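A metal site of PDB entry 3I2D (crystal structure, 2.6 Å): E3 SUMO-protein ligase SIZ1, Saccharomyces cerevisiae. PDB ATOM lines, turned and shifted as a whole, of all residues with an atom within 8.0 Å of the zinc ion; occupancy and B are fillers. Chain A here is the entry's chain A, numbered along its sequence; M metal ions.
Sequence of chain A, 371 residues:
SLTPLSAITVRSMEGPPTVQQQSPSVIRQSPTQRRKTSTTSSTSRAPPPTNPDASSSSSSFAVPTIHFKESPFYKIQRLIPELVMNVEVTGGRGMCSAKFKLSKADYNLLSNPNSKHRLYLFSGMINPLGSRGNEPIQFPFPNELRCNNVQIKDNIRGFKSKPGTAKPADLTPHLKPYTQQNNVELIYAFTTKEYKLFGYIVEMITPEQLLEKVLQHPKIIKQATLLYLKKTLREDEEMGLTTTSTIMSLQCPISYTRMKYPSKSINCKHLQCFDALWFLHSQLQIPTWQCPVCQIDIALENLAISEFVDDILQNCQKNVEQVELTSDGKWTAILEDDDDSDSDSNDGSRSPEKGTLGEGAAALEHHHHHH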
ATOM      1  N   SER A 263      11.566  14.155   5.543  1.00  0.00           N
ATOM      2  CA  SER A 263      10.897  14.684   4.387  1.00  0.00           C
ATOM      3  C   SER A 263       9.757  15.647   4.654  1.00  0.00           C
ATOM      4  O   SER A 263       9.363  15.887   5.785  1.00  0.00           O
ATOM      5  CB  SER A 263      10.427  13.521   3.520  1.00  0.00           C
ATOM      6  OG  SER A 263       9.879  12.485   4.309  1.00  0.00           O
ATOM      7  N   LYS A 264       9.239  16.204   3.577  1.00  0.00           N
ATOM      8  CA  LYS A 264       8.143  17.160   3.632  1.00  0.00           C
ATOM      9  C   LYS A 264       7.891  17.563   2.197  1.00  0.00           C
ATOM     10  O   LYS A 264       8.745  17.335   1.343  1.00  0.00           O
ATOM     11  CB  LYS A 264       8.538  18.394   4.461  1.00  0.00           C
ATOM     12  CG  LYS A 264       9.765  19.142   3.947  1.00  0.00           C
ATOM     13  CD  LYS A 264      10.322  20.079   5.026  1.00  0.00           C
ATOM     14  CE  LYS A 264      11.569  20.797   4.533  1.00  0.00           C
ATOM     15  NZ  LYS A 264      12.241  21.529   5.654  1.00  0.00           N
ATOM     16  N   SER A 265       6.723  18.146   1.928  1.00  0.00           N
ATOM     17  CA  SER A 265       6.382  18.610   0.589  1.00  0.00           C
ATOM     18  C   SER A 265       7.305  19.761   0.304  1.00  0.00           C
ATOM     19  O   SER A 265       7.691  20.505   1.229  1.00  0.00           O
ATOM     20  CB  SER A 265       4.937  19.115   0.525  1.00  0.00           C
ATOM     21  OG  SER A 265       4.573  19.525  -0.789  1.00  0.00           O
ATOM     22  N   ILE A 266       7.671  19.935  -0.959  1.00  0.00           N
ATOM     23  CA  ILE A 266       8.524  21.061  -1.318  1.00  0.00           C
ATOM     24  C   ILE A 266       7.708  22.331  -1.054  1.00  0.00           C
ATOM     25  O   ILE A 266       8.255  23.439  -0.942  1.00  0.00           O
ATOM     26  CB  ILE A 266       8.931  20.955  -2.792  1.00  0.00           C
ATOM     27  CG1 ILE A 266       7.689  21.036  -3.683  1.00  0.00           C
ATOM     28  CG2 ILE A 266       9.670  19.632  -3.018  1.00  0.00           C
ATOM     29  CD1 ILE A 266       7.982  20.829  -5.151  1.00  0.00           C
ATOM     30  N   ASN A 267       6.394  22.150  -0.915  1.00  0.00           N
ATOM     31  CA  ASN A 267       5.477  23.240  -0.626  1.00  0.00           C
ATOM     32  C   ASN A 267       5.370  23.533   0.881  1.00  0.00           C
ATOM     33  O   ASN A 267       4.659  24.459   1.278  1.00  0.00           O
ATOM     34  CB  ASN A 267       4.084  22.926  -1.161  1.00  0.00           C
ATOM     35  CG  ASN A 267       4.068  22.804  -2.672  1.00  0.00           C
ATOM     36  OD1 ASN A 267       4.940  23.328  -3.357  1.00  0.00           O
ATOM     37  ND2 ASN A 267       3.049  22.122  -3.204  1.00  0.00           N
ATOM     38  N   CYS A 268       6.056  22.752   1.707  1.00  0.00           N
ATOM     39  CA  CYS A 268       5.981  22.984   3.140  1.00  0.00           C
ATOM     40  C   CYS A 268       6.884  24.130   3.611  1.00  0.00           C
ATOM     41  O   CYS A 268       8.051  24.230   3.231  1.00  0.00           O
ATOM     42  CB  CYS A 268       6.313  21.694   3.919  1.00  0.00           C
ATOM     43  SG  CYS A 268       4.933  20.477   4.089  1.00  0.00           S
ATOM     44  N   LYS A 269       6.313  25.009   4.429  1.00  0.00           N
ATOM     45  CA  LYS A 269       7.034  26.148   4.973  1.00  0.00           C
ATOM     46  C   LYS A 269       7.378  25.863   6.427  1.00  0.00           C
ATOM     47  O   LYS A 269       6.717  26.338   7.350  1.00  0.00           O
ATOM     48  CB  LYS A 269       6.179  27.412   4.910  1.00  0.00           C
ATOM     49  CG  LYS A 269       6.169  28.113   3.560  1.00  0.00           C
ATOM     50  CD  LYS A 269       5.277  27.434   2.533  1.00  0.00           C
ATOM     51  CE  LYS A 269       5.413  28.124   1.179  1.00  0.00           C
ATOM     52  NZ  LYS A 269       5.220  29.599   1.267  1.00  0.00           N
ATOM     53  N   HIS A 270       8.409  25.057   6.631  1.00  0.00           N
ATOM     54  CA  HIS A 270       8.844  24.727   7.980  1.00  0.00           C
ATOM     55  C   HIS A 270      10.026  23.777   7.922  1.00  0.00           C
ATOM     56  O   HIS A 270      10.180  23.000   6.970  1.00  0.00           O
ATOM     57  CB  HIS A 270       7.682  24.136   8.826  1.00  0.00           C
ATOM     58  CG  HIS A 270       7.085  22.878   8.271  1.00  0.00           C
ATOM     59  ND1 HIS A 270       7.722  21.657   8.333  1.00  0.00           N
ATOM     60  CD2 HIS A 270       5.903  22.646   7.646  1.00  0.00           C
ATOM     61  CE1 HIS A 270       6.962  20.731   7.773  1.00  0.00           C
ATOM     62  NE2 HIS A 270       5.854  21.301   7.348  1.00  0.00           N
ATOM     63  N   LEU A 271      10.879  23.863   8.936  1.00  0.00           N
ATOM     64  CA  LEU A 271      12.069  23.044   9.036  1.00  0.00           C
ATOM     65  C   LEU A 271      11.778  21.597   9.408  1.00  0.00           C
ATOM     66  O   LEU A 271      12.372  20.670   8.827  1.00  0.00           O
ATOM     67  CB  LEU A 271      12.984  23.658  10.092  1.00  0.00           C
ATOM     68  CG  LEU A 271      14.360  24.110   9.628  1.00  0.00           C
ATOM     69  CD1 LEU A 271      14.272  24.887   8.323  1.00  0.00           C
ATOM     70  CD2 LEU A 271      14.966  24.961  10.736  1.00  0.00           C
ATOM     71  N   GLN A 272      10.865  21.389  10.358  1.00  0.00           N
ATOM     72  CA  GLN A 272      10.500  20.054  10.820  1.00  0.00           C
ATOM     73  C   GLN A 272      10.056  19.122   9.707  1.00  0.00           C
ATOM     74  O   GLN A 272       9.123  19.419   8.968  1.00  0.00           O
ATOM     75  CB  GLN A 272       9.402  20.141  11.889  1.00  0.00           C
ATOM     76  CG  GLN A 272       8.993  18.788  12.537  1.00  0.00           C
ATOM     77  CD  GLN A 272      10.185  17.973  13.037  1.00  0.00           C
ATOM     78  OE1 GLN A 272      11.092  18.505  13.688  1.00  0.00           O
ATOM     79  NE2 GLN A 272      10.190  16.675  12.734  1.00  0.00           N
ATOM     80  N   CYS A 273      10.746  17.983   9.587  1.00  0.00           N
ATOM     81  CA  CYS A 273      10.404  16.993   8.591  1.00  0.00           C
ATOM     82  C   CYS A 273       9.710  15.861   9.329  1.00  0.00           C
ATOM     83  O   CYS A 273       9.504  15.940  10.544  1.00  0.00           O
ATOM     84  CB  CYS A 273      11.650  16.452   7.894  1.00  0.00           C
ATOM     85  SG  CYS A 273      12.556  17.698   6.974  1.00  0.00           S
ATOM     86  N   PHE A 274       9.352  14.818   8.603  1.00  0.00           N
ATOM     87  CA  PHE A 274       8.719  13.650   9.195  1.00  0.00           C
ATOM     88  C   PHE A 274       9.225  12.465   8.395  1.00  0.00           C
ATOM     89  O   PHE A 274       9.719  12.636   7.286  1.00  0.00           O
ATOM     90  CB  PHE A 274       7.197  13.752   9.113  1.00  0.00           C
ATOM     91  CG  PHE A 274       6.695  14.030   7.747  1.00  0.00           C
ATOM     92  CD1 PHE A 274       6.427  15.344   7.351  1.00  0.00           C
ATOM     93  CD2 PHE A 274       6.504  12.999   6.830  1.00  0.00           C
ATOM     94  CE1 PHE A 274       5.980  15.623   6.070  1.00  0.00           C
ATOM     95  CE2 PHE A 274       6.063  13.271   5.552  1.00  0.00           C
ATOM     96  CZ  PHE A 274       5.795  14.590   5.169  1.00  0.00           C
ATOM     97  N   GLN A 290      -2.131  14.749   4.240  1.00  0.00           N
ATOM     98  CA  GLN A 290      -1.936  16.031   4.910  1.00  0.00           C
ATOM     99  C   GLN A 290      -0.658  15.957   5.706  1.00  0.00           C
ATOM    100  O   GLN A 290      -0.385  14.961   6.373  1.00  0.00           O
ATOM    101  CB  GLN A 290      -3.051  16.320   5.893  1.00  0.00           C
ATOM    102  CG  GLN A 290      -4.292  16.860   5.281  1.00  0.00           C
ATOM    103  CD  GLN A 290      -5.268  17.343   6.325  1.00  0.00           C
ATOM    104  OE1 GLN A 290      -6.173  18.124   6.031  1.00  0.00           O
ATOM    105  NE2 GLN A 290      -5.092  16.872   7.567  1.00  0.00           N
ATOM    106  N   CYS A 291       0.134  17.021   5.659  1.00  0.00           N
ATOM    107  CA  CYS A 291       1.374  17.047   6.373  1.00  0.00           C
ATOM    108  C   CYS A 291       1.088  16.921   7.876  1.00  0.00           C
ATOM    109  O   CYS A 291       0.214  17.595   8.391  1.00  0.00           O
ATOM    110  CB  CYS A 291       2.124  18.345   6.071  1.00  0.00           C
ATOM    111  SG  CYS A 291       3.697  18.547   6.922  1.00  0.00           S
ATOM    112  N   PRO A 292       1.829  16.038   8.577  1.00  0.00           N
ATOM    113  CA  PRO A 292       1.688  15.807  10.025  1.00  0.00           C
ATOM    114  C   PRO A 292       2.119  17.015  10.849  1.00  0.00           C
ATOM    115  O   PRO A 292       1.721  17.166  12.011  1.00  0.00           O
ATOM    116  CB  PRO A 292       2.615  14.624  10.292  1.00  0.00           C
ATOM    117  CG  PRO A 292       2.737  13.940   8.962  1.00  0.00           C
ATOM    118  CD  PRO A 292       2.808  15.093   8.002  1.00  0.00           C
ATOM    119  N   VAL A 293       2.936  17.868  10.254  1.00  0.00           N
ATOM    120  CA  VAL A 293       3.444  19.050  10.920  1.00  0.00           C
ATOM    121  C   VAL A 293       2.573  20.320  10.738  1.00  0.00           C
ATOM    122  O   VAL A 293       2.153  20.939  11.721  1.00  0.00           O
ATOM    123  CB  VAL A 293       4.896  19.343  10.455  1.00  0.00           C
ATOM    124  CG1 VAL A 293       5.480  20.488  11.236  1.00  0.00           C
ATOM    125  CG2 VAL A 293       5.748  18.100  10.640  1.00  0.00           C
ATOM    126  N   CYS A 294       2.300  20.699   9.490  1.00  0.00           N
ATOM    127  CA  CYS A 294       1.509  21.892   9.156  1.00  0.00           C
ATOM    128  C   CYS A 294       0.097  21.619   8.626  1.00  0.00           C
ATOM    129  O   CYS A 294      -0.629  22.529   8.253  1.00  0.00           O
ATOM    130  CB  CYS A 294       2.254  22.728   8.114  1.00  0.00           C
ATOM    131  SG  CYS A 294       2.416  21.917   6.499  1.00  0.00           S
ATOM    132  N   GLN A 295      -0.273  20.345   8.578  1.00  0.00           N
ATOM    133  CA  GLN A 295      -1.574  19.915   8.107  1.00  0.00           C
ATOM    134  C   GLN A 295      -1.981  20.305   6.701  1.00  0.00           C
ATOM    135  O   GLN A 295      -3.123  20.040   6.313  1.00  0.00           O
ATOM    136  CB  GLN A 295      -2.681  20.394   9.054  1.00  0.00           C
ATOM    137  CG  GLN A 295      -2.615  19.833  10.451  1.00  0.00           C
ATOM    138  CD  GLN A 295      -1.456  20.387  11.246  1.00  0.00           C
ATOM    139  OE1 GLN A 295      -1.210  21.592  11.263  1.00  0.00           O
ATOM    140  NE2 GLN A 295      -0.732  19.496  11.934  1.00  0.00           N
ATOM    141  N   ILE A 296      -1.109  20.926   5.913  1.00  0.00           N
ATOM    142  CA  ILE A 296      -1.518  21.289   4.549  1.00  0.00           C
ATOM    143  C   ILE A 296      -1.707  20.067   3.676  1.00  0.00           C
ATOM    144  O   ILE A 296      -1.354  18.953   4.062  1.00  0.00           O
ATOM    145  CB  ILE A 296      -0.503  22.226   3.832  1.00  0.00           C
ATOM    146  CG1 ILE A 296       0.656  21.423   3.240  1.00  0.00           C
ATOM    147  CG2 ILE A 296       0.021  23.252   4.795  1.00  0.00           C
ATOM    148  CD1 ILE A 296       1.550  22.242   2.305  1.00  0.00           C
ATOM    149  N   ASP A 297      -2.267  20.271   2.489  1.00  0.00           N
ATOM    150  CA  ASP A 297      -2.467  19.177   1.545  1.00  0.00           C
ATOM    151  C   ASP A 297      -1.188  18.974   0.779  1.00  0.00           C
ATOM    152  O   ASP A 297      -0.602  19.925   0.242  1.00  0.00           O
ATOM    153  CB  ASP A 297      -3.562  19.516   0.550  1.00  0.00           C
ATOM    154  CG  ASP A 297      -4.801  18.727   0.796  1.00  0.00           C
ATOM    155  OD1 ASP A 297      -5.375  18.879   1.904  1.00  0.00           O
ATOM    156  OD2 ASP A 297      -5.202  17.951  -0.107  1.00  0.00           O
ATOM    157  N   ILE A 298      -0.737  17.719   0.726  1.00  0.00           N
ATOM    158  CA  ILE A 298       0.487  17.400   0.002  1.00  0.00           C
ATOM    159  C   ILE A 298       0.217  16.236  -0.927  1.00  0.00           C
ATOM    160  O   ILE A 298      -0.609  15.376  -0.628  1.00  0.00           O
ATOM    161  CB  ILE A 298       1.635  17.040   0.968  1.00  0.00           C
ATOM    162  CG1 ILE A 298       1.364  15.714   1.649  1.00  0.00           C
ATOM    163  CG2 ILE A 298       1.802  18.101   2.042  1.00  0.00           C
ATOM    164  CD1 ILE A 298       2.418  15.417   2.696  1.00  0.00           C
HETATM  165 ZN    ZN M   1       4.281  20.632   6.097  1.00  0.00          ZN
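SG of Cys 268 sits close to N of Ser 265 (3.6 Å). The backbone carbonyl oxygen (O) of His 270 sits at hydrogen-bond distance from the side-chain amino group (NZ) of Lys 264 (2.9 Å). A ring nitrogen (ND1) of His 270 sits at hydrogen-bond distance from the backbone carbonyl oxygen (O) of Gln 272, at 2.7 Å. The backbone NH (N) of Ile 296 sits close to the side-chain sulfur (SG) of Cys 294 (3.7 Å). The backbone NH of Val 293 lies close to the side-chain sulfur of Cys 291 (3.5 Å). The backbone NH of Cys 291 is in hydrogen-bond range of the backbone carbonyl oxygen of Ile 296 (2.9 Å).
Within 4 Å of the zinc ion: Cys 268, His 270, Cys 291 and Cys 294. The nearest printed residue that does not touch the zinc ion is Val 293 (4.6 Å).
The zinc ion is bound by SG of Cys 268 (2.1 Å), NE2 of His 270 (2.1 Å), SG of Cys 294 (2.3 Å) and SG of Cys 291 (2.3 Å).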
